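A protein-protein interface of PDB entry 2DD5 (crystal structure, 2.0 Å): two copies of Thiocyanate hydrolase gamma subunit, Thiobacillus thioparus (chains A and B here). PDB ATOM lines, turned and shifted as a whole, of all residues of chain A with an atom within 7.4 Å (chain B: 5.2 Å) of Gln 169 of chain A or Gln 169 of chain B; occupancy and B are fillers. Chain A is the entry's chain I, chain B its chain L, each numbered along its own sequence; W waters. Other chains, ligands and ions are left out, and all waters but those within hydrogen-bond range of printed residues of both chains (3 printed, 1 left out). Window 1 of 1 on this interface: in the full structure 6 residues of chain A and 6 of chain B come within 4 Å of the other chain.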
ATOM      1  N   ARG A 160     -33.062  10.978  -2.000  1.00  0.00           N
ATOM      2  CA  ARG A 160     -31.680  10.583  -2.285  1.00  0.00           C
ATOM      3  C   ARG A 160     -31.087  11.452  -3.383  1.00  0.00           C
ATOM      4  O   ARG A 160     -29.934  11.886  -3.304  1.00  0.00           O
ATOM      5  CB  ARG A 160     -31.626   9.118  -2.726  1.00  0.00           C
ATOM      6  CG  ARG A 160     -32.081   8.115  -1.671  1.00  0.00           C
ATOM      7  CD  ARG A 160     -30.917   7.616  -0.856  1.00  0.00           C
ATOM      8  NE  ARG A 160     -31.338   6.728   0.223  1.00  0.00           N
ATOM      9  CZ  ARG A 160     -30.497   6.156   1.078  1.00  0.00           C
ATOM     10  NH1 ARG A 160     -29.194   6.379   0.968  1.00  0.00           N
ATOM     11  NH2 ARG A 160     -30.955   5.384   2.054  1.00  0.00           N
ATOM     12  N   GLN A 161     -31.882  11.706  -4.415  1.00  0.00           N
ATOM     13  CA  GLN A 161     -31.426  12.515  -5.531  1.00  0.00           C
ATOM     14  C   GLN A 161     -31.268  13.983  -5.141  1.00  0.00           C
ATOM     15  O   GLN A 161     -30.268  14.610  -5.481  1.00  0.00           O
ATOM     16  CB  GLN A 161     -32.389  12.361  -6.713  1.00  0.00           C
ATOM     17  CG  GLN A 161     -32.443  10.933  -7.292  1.00  0.00           C
ATOM     18  CD  GLN A 161     -33.241   9.941  -6.439  1.00  0.00           C
ATOM     19  OE1 GLN A 161     -33.928  10.320  -5.492  1.00  0.00           O
ATOM     20  NE2 GLN A 161     -33.157   8.661  -6.790  1.00  0.00           N
ATOM     21  N   LEU A 163     -30.814  15.234  -2.088  1.00  0.00           N
ATOM     22  CA  LEU A 163     -29.695  15.328  -1.156  1.00  0.00           C
ATOM     23  C   LEU A 163     -28.360  15.241  -1.891  1.00  0.00           C
ATOM     24  O   LEU A 163     -27.404  15.924  -1.527  1.00  0.00           O
ATOM     25  CB  LEU A 163     -29.787  14.224  -0.100  1.00  0.00           C
ATOM     26  CG  LEU A 163     -30.921  14.367   0.920  1.00  0.00           C
ATOM     27  CD1 LEU A 163     -30.894  13.191   1.884  1.00  0.00           C
ATOM     28  CD2 LEU A 163     -30.765  15.681   1.682  1.00  0.00           C
ATOM     29  N   ALA A 164     -28.296  14.414  -2.935  1.00  0.00           N
ATOM     30  CA  ALA A 164     -27.062  14.270  -3.704  1.00  0.00           C
ATOM     31  C   ALA A 164     -26.715  15.585  -4.394  1.00  0.00           C
ATOM     32  O   ALA A 164     -25.542  15.933  -4.528  1.00  0.00           O
ATOM     33  CB  ALA A 164     -27.199  13.141  -4.739  1.00  0.00           C
ATOM     34  N   PHE A 166     -27.319  18.411  -3.201  1.00  0.00           N
ATOM     35  CA  PHE A 166     -26.813  19.235  -2.105  1.00  0.00           C
ATOM     36  C   PHE A 166     -25.425  18.748  -1.680  1.00  0.00           C
ATOM     37  O   PHE A 166     -24.778  19.363  -0.836  1.00  0.00           O
ATOM     38  CB  PHE A 166     -27.764  19.162  -0.907  1.00  0.00           C
ATOM     39  CG  PHE A 166     -28.899  20.148  -0.964  1.00  0.00           C
ATOM     40  CD1 PHE A 166     -28.691  21.487  -0.648  1.00  0.00           C
ATOM     41  CD2 PHE A 166     -30.180  19.736  -1.319  1.00  0.00           C
ATOM     42  CE1 PHE A 166     -29.746  22.399  -0.680  1.00  0.00           C
ATOM     43  CE2 PHE A 166     -31.240  20.641  -1.356  1.00  0.00           C
ATOM     44  CZ  PHE A 166     -31.020  21.976  -1.034  1.00  0.00           C
ATOM     45  N   GLY A 167     -24.979  17.637  -2.265  1.00  0.00           N
ATOM     46  CA  GLY A 167     -23.669  17.097  -1.936  1.00  0.00           C
ATOM     47  C   GLY A 167     -23.661  16.119  -0.770  1.00  0.00           C
ATOM     48  O   GLY A 167     -22.610  15.860  -0.180  1.00  0.00           O
ATOM     49  N   LEU A 168     -24.826  15.570  -0.437  1.00  0.00           N
ATOM     50  CA  LEU A 168     -24.931  14.625   0.666  1.00  0.00           C
ATOM     51  C   LEU A 168     -25.413  13.249   0.217  1.00  0.00           C
ATOM     52  O   LEU A 168     -26.464  13.118  -0.405  1.00  0.00           O
ATOM     53  CB  LEU A 168     -25.878  15.165   1.741  1.00  0.00           C
ATOM     54  CG  LEU A 168     -26.202  14.190   2.877  1.00  0.00           C
ATOM     55  CD1 LEU A 168     -24.923  13.809   3.617  1.00  0.00           C
ATOM     56  CD2 LEU A 168     -27.210  14.829   3.822  1.00  0.00           C
ATOM     57  N   GLN A 169     -24.638  12.224   0.552  1.00  0.00           N
ATOM     58  CA  GLN A 169     -24.984  10.853   0.198  1.00  0.00           C
ATOM     59  C   GLN A 169     -24.825   9.970   1.431  1.00  0.00           C
ATOM     60  O   GLN A 169     -23.843  10.096   2.159  1.00  0.00           O
ATOM     61  CB  GLN A 169     -24.064  10.357  -0.918  1.00  0.00           C
ATOM     62  CG  GLN A 169     -24.483   9.046  -1.553  1.00  0.00           C
ATOM     63  CD  GLN A 169     -23.578   8.654  -2.713  1.00  0.00           C
ATOM     64  OE1 GLN A 169     -22.461   8.174  -2.511  1.00  0.00           O
ATOM     65  NE2 GLN A 169     -24.056   8.872  -3.935  1.00  0.00           N
ATOM     66  N   LEU A 170     -25.798   9.095   1.669  1.00  0.00           N
ATOM     67  CA  LEU A 170     -25.753   8.175   2.804  1.00  0.00           C
ATOM     68  C   LEU A 170     -25.768   6.738   2.290  1.00  0.00           C
ATOM     69  O   LEU A 170     -26.219   6.478   1.172  1.00  0.00           O
ATOM     70  CB  LEU A 170     -26.968   8.374   3.723  1.00  0.00           C
ATOM     71  CG  LEU A 170     -27.043   9.549   4.707  1.00  0.00           C
ATOM     72  CD1 LEU A 170     -25.863   9.483   5.660  1.00  0.00           C
ATOM     73  CD2 LEU A 170     -27.049  10.865   3.961  1.00  0.00           C
ATOM     74  N   PRO A 171     -25.264   5.782   3.096  1.00  0.00           N
ATOM     75  CA  PRO A 171     -25.258   4.381   2.666  1.00  0.00           C
ATOM     76  C   PRO A 171     -26.688   3.986   2.316  1.00  0.00           C
ATOM     77  O   PRO A 171     -27.637   4.512   2.896  1.00  0.00           O
ATOM     78  CB  PRO A 171     -24.733   3.645   3.897  1.00  0.00           C
ATOM     79  CG  PRO A 171     -23.785   4.649   4.494  1.00  0.00           C
ATOM     80  CD  PRO A 171     -24.573   5.942   4.388  1.00  0.00           C
ATOM     81  N   SER A 172     -26.846   3.068   1.369  1.00  0.00           N
ATOM     82  CA  SER A 172     -28.173   2.648   0.945  1.00  0.00           C
ATOM     83  C   SER A 172     -28.983   1.969   2.043  1.00  0.00           C
ATOM     84  O   SER A 172     -30.213   2.017   2.026  1.00  0.00           O
ATOM     85  CB  SER A 172     -28.065   1.718  -0.269  1.00  0.00           C
ATOM     86  OG  SER A 172     -27.369   0.532   0.062  1.00  0.00           O
ATOM     87  N   GLU A 173     -28.305   1.343   3.000  1.00  0.00           N
ATOM     88  CA  GLU A 173     -29.006   0.660   4.084  1.00  0.00           C
ATOM     89  C   GLU A 173     -29.484   1.635   5.158  1.00  0.00           C
ATOM     90  O   GLU A 173     -30.350   1.302   5.963  1.00  0.00           O
ATOM     91  CB  GLU A 173     -28.107  -0.403   4.731  1.00  0.00           C
ATOM     92  CG  GLU A 173     -26.914   0.163   5.486  1.00  0.00           C
ATOM     93  CD  GLU A 173     -25.677   0.323   4.618  1.00  0.00           C
ATOM     94  OE1 GLU A 173     -25.812   0.397   3.372  1.00  0.00           O
ATOM     95  OE2 GLU A 173     -24.564   0.385   5.190  1.00  0.00           O
ATOM     96  N   ILE A 176     -33.291   6.895   5.287  1.00  0.00           N
ATOM     97  CA  ILE A 176     -33.411   8.338   5.118  1.00  0.00           C
ATOM     98  C   ILE A 176     -34.871   8.610   5.438  1.00  0.00           C
ATOM     99  O   ILE A 176     -35.761   8.002   4.840  1.00  0.00           O
ATOM    100  CB  ILE A 176     -33.153   8.814   3.670  1.00  0.00           C
ATOM    101  CG1 ILE A 176     -31.682   8.634   3.296  1.00  0.00           C
ATOM    102  CG2 ILE A 176     -33.552  10.290   3.541  1.00  0.00           C
ATOM    103  CD1 ILE A 176     -30.742   9.536   4.053  1.00  0.00           C
ATOM    104  N   VAL A 217     -30.120  18.979   4.934  1.00  0.00           N
ATOM    105  CA  VAL A 217     -29.546  18.866   3.596  1.00  0.00           C
ATOM    106  C   VAL A 217     -28.019  18.773   3.626  1.00  0.00           C
ATOM    107  O   VAL A 217     -27.377  18.578   2.594  1.00  0.00           O
ATOM    108  CB  VAL A 217     -29.974  20.045   2.687  1.00  0.00           C
ATOM    109  CG1 VAL A 217     -31.499  20.094   2.590  1.00  0.00           C
ATOM    110  CG2 VAL A 217     -29.425  21.358   3.222  1.00  0.00           C
ATOM    111  N   VAL A 219     -24.482  17.676   6.512  1.00  0.00           N
ATOM    112  CA  VAL A 219     -24.083  17.076   7.782  1.00  0.00           C
ATOM    113  C   VAL A 219     -22.906  17.900   8.274  1.00  0.00           C
ATOM    114  O   VAL A 219     -22.148  18.448   7.471  1.00  0.00           O
ATOM    115  CB  VAL A 219     -23.652  15.587   7.645  1.00  0.00           C
ATOM    116  CG1 VAL A 219     -24.877  14.721   7.365  1.00  0.00           C
ATOM    117  CG2 VAL A 219     -22.603  15.435   6.544  1.00  0.00           C
ATOM    118  N   ARG B 160     -25.223  10.634 -10.949  1.00  0.00           N
ATOM    119  CA  ARG B 160     -25.450  10.075  -9.614  1.00  0.00           C
ATOM    120  C   ARG B 160     -26.932   9.944  -9.320  1.00  0.00           C
ATOM    121  O   ARG B 160     -27.386   8.942  -8.762  1.00  0.00           O
ATOM    122  CB  ARG B 160     -24.826  10.978  -8.546  1.00  0.00           C
ATOM    123  CG  ARG B 160     -23.323  11.125  -8.654  1.00  0.00           C
ATOM    124  CD  ARG B 160     -22.624  10.094  -7.816  1.00  0.00           C
ATOM    125  NE  ARG B 160     -21.172  10.183  -7.932  1.00  0.00           N
ATOM    126  CZ  ARG B 160     -20.332   9.451  -7.208  1.00  0.00           C
ATOM    127  NH1 ARG B 160     -20.813   8.591  -6.322  1.00  0.00           N
ATOM    128  NH2 ARG B 160     -19.022   9.570  -7.373  1.00  0.00           N
ATOM    129  N   LEU B 163     -28.478   7.254 -11.763  1.00  0.00           N
ATOM    130  CA  LEU B 163     -28.081   5.911 -11.346  1.00  0.00           C
ATOM    131  C   LEU B 163     -28.811   5.498 -10.064  1.00  0.00           C
ATOM    132  O   LEU B 163     -29.215   4.341  -9.915  1.00  0.00           O
ATOM    133  CB  LEU B 163     -26.564   5.843 -11.138  1.00  0.00           C
ATOM    134  CG  LEU B 163     -25.727   5.851 -12.422  1.00  0.00           C
ATOM    135  CD1 LEU B 163     -24.247   5.844 -12.082  1.00  0.00           C
ATOM    136  CD2 LEU B 163     -26.082   4.628 -13.266  1.00  0.00           C
ATOM    137  N   GLY B 167     -31.232   2.360  -8.805  1.00  0.00           N
ATOM    138  CA  GLY B 167     -30.866   1.594  -7.627  1.00  0.00           C
ATOM    139  C   GLY B 167     -29.372   1.359  -7.477  1.00  0.00           C
ATOM    140  O   GLY B 167     -28.950   0.469  -6.733  1.00  0.00           O
ATOM    141  N   LEU B 168     -28.568   2.154  -8.175  1.00  0.00           N
ATOM    142  CA  LEU B 168     -27.119   2.017  -8.102  1.00  0.00           C
ATOM    143  C   LEU B 168     -26.462   3.244  -7.484  1.00  0.00           C
ATOM    144  O   LEU B 168     -26.624   4.366  -7.961  1.00  0.00           O
ATOM    145  CB  LEU B 168     -26.529   1.782  -9.492  1.00  0.00           C
ATOM    146  CG  LEU B 168     -25.000   1.763  -9.565  1.00  0.00           C
ATOM    147  CD1 LEU B 168     -24.439   0.666  -8.654  1.00  0.00           C
ATOM    148  CD2 LEU B 168     -24.570   1.544 -11.006  1.00  0.00           C
ATOM    149  N   GLN B 169     -25.708   3.015  -6.418  1.00  0.00           N
ATOM    150  CA  GLN B 169     -25.011   4.088  -5.737  1.00  0.00           C
ATOM    151  C   GLN B 169     -23.564   3.672  -5.502  1.00  0.00           C
ATOM    152  O   GLN B 169     -23.284   2.518  -5.176  1.00  0.00           O
ATOM    153  CB  GLN B 169     -25.710   4.387  -4.411  1.00  0.00           C
ATOM    154  CG  GLN B 169     -25.074   5.473  -3.576  1.00  0.00           C
ATOM    155  CD  GLN B 169     -25.962   5.891  -2.414  1.00  0.00           C
ATOM    156  OE1 GLN B 169     -26.896   6.685  -2.575  1.00  0.00           O
ATOM    157  NE2 GLN B 169     -25.683   5.348  -1.240  1.00  0.00           N
ATOM    158  N   LEU B 170     -22.649   4.613  -5.699  1.00  0.00           N
ATOM    159  CA  LEU B 170     -21.233   4.357  -5.495  1.00  0.00           C
ATOM    160  C   LEU B 170     -20.645   5.380  -4.537  1.00  0.00           C
ATOM    161  O   LEU B 170     -21.175   6.480  -4.395  1.00  0.00           O
ATOM    162  CB  LEU B 170     -20.472   4.426  -6.816  1.00  0.00           C
ATOM    163  CG  LEU B 170     -20.573   3.219  -7.750  1.00  0.00           C
ATOM    164  CD1 LEU B 170     -21.840   3.262  -8.578  1.00  0.00           C
ATOM    165  CD2 LEU B 170     -19.371   3.236  -8.649  1.00  0.00           C
ATOM    166  N   PRO B 171     -19.544   5.022  -3.857  1.00  0.00           N
ATOM    167  CA  PRO B 171     -18.896   5.938  -2.916  1.00  0.00           C
ATOM    168  C   PRO B 171     -18.636   7.268  -3.607  1.00  0.00           C
ATOM    169  O   PRO B 171     -18.399   7.312  -4.819  1.00  0.00           O
ATOM    170  CB  PRO B 171     -17.607   5.205  -2.556  1.00  0.00           C
ATOM    171  CG  PRO B 171     -18.049   3.767  -2.568  1.00  0.00           C
ATOM    172  CD  PRO B 171     -18.883   3.704  -3.846  1.00  0.00           C
ATOM    173  N   SER B 172     -18.678   8.346  -2.834  1.00  0.00           N
ATOM    174  CA  SER B 172     -18.467   9.685  -3.366  1.00  0.00           C
ATOM    175  C   SER B 172     -17.078   9.910  -3.960  1.00  0.00           C
ATOM    176  O   SER B 172     -16.922  10.723  -4.872  1.00  0.00           O
ATOM    177  CB  SER B 172     -18.732  10.720  -2.270  1.00  0.00           C
ATOM    178  OG  SER B 172     -17.868  10.520  -1.166  1.00  0.00           O
HETATM  179  O   HOH W   1     -26.846   8.907  -4.532  1.00  0.00           O
HETATM  180  O   HOH W   2     -27.748   8.693  -0.303  1.00  0.00           O
HETATM  181  O   HOH W   3     -28.622  10.408  -5.992  1.00  0.00           O
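The guanidinium group (NH1) of Arg 160 of chain A sits at hydrogen-bond distance from the backbone carbonyl oxygen (O) of Leu 170 of chain A (3.0 Å). The backbone carbonyl oxygen (O) of Pro 171 of chain A is in hydrogen-bond range of the guanidinium group (NH1) of Arg 160 of chain A (3.1 Å). O of Ser 172 of chain A is in hydrogen-bond range of NH2 of Arg 160 of chain A (3.4 Å). The guanidinium group (NH1) of Arg 160 of chain B sits at hydrogen-bond distance from the backbone carbonyl oxygen (O) of Leu 170 of chain B (2.9 Å). O of Ser 172 of chain B lies within hydrogen-bond range of NH2 of Arg 160 of chain B (3.5 Å).
Water W2 lies within hydrogen-bond range of N of Leu 170 of chain A (2.8 Å), NH1 of Arg 160 of chain A (3.0 Å) and OE1 of Gln 169 of chain B (3.1 Å). Water W1 lies within hydrogen-bond range of the side-chain amide nitrogen (NE2) of Gln 169 of chain A and the side-chain amide oxygen (OE1) of Gln 169 of chain B. Water W3 bridges the backbone carbonyl oxygen of Arg 160 of chain A and the backbone carbonyl oxygen of Arg 160 of chain B.
Among the printed residues, merely in contact across the chains: Gln 169 of chain A with Gln 169 of chain B, Gln 169 of chain A with Ser 172 of chain B, Pro 171 of chain A with Gln 169 of chain B and Ser 172 of chain A with Gln 169 of chain B.
Gln 161 of chain A touches none of the printed residues of chain B. Of the printed residues of chain B, Gln 169 of chain A touches Gln 169 (3.5 Å), Leu 170 (2.8 Å) and Ser 172 (3.8 Å). Of the printed residues of chain B, Leu 170 of chain A touches Gln 169 (2.7 Å). Of the printed residues of chain B, Pro 171 of chain A touches Gln 169 (3.9 Å). Val 219 of chain A touches none of the printed residues of chain B. Of chain A, only Gln 169 (3.5 Å), Leu 170 (2.7 Å), Pro 171 (3.9 Å) and Ser 172 (3.7 Å) come within 4 Å of Gln 169 of chain B. Of the printed residues of chain A, Leu 170 of chain B touches Gln 169. Of the printed residues of chain A, Ser 172 of chain B touches Gln 169 (3.8 Å). The nearest residue of chain B that does not touch Gln 169 of chain A is Arg 160 of chain B (4.04 Å). The nearest printed residue of chain B that does not touch Ser 172 of chain A is Gly 167 of chain B (6.6 Å).
Gln 169 of chain B touches its own counterpart, Gln 169 of chain A. Gln 169 of chain A touches Leu 170 of chain B, and with the chains exchanged Leu 170 of chain A touches Gln 169 of chain B. Gln 169 of chain A touches Ser 172 of chain B, and with the chains exchanged Ser 172 of chain A touches Gln 169 of chain B. Pro 171 of chain A touches Gln 169 of chain B, but with the chains exchanged Gln 169 of chain A does not touch Pro 171 of chain B (4.1 Å). Of the 6 pairs that touch across the chains among the printed residues, 5 have their exchanged pair printed and touching as well.
The backbone carbonyl oxygen (O) of Leu 170 of chain B lies close to the side-chain amide oxygen (OE1) of Gln 169 of chain A (2.8 Å). The backbone carbonyl oxygen of Leu 170 of chain A sits at hydrogen-bond distance from the side-chain amide nitrogen of Gln 169 of chain B, 2.7 Å away.
Printed residues of chain B that touch a printed residue of chain A: Gln 169, Leu 170 and Ser 172. Among the printed residues, 6 pairs touch across the chains. Among the printed residues, no Asp or Glu carboxylate lies within 4 Å of a Lys or Arg side-chain nitrogen of the other chain.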
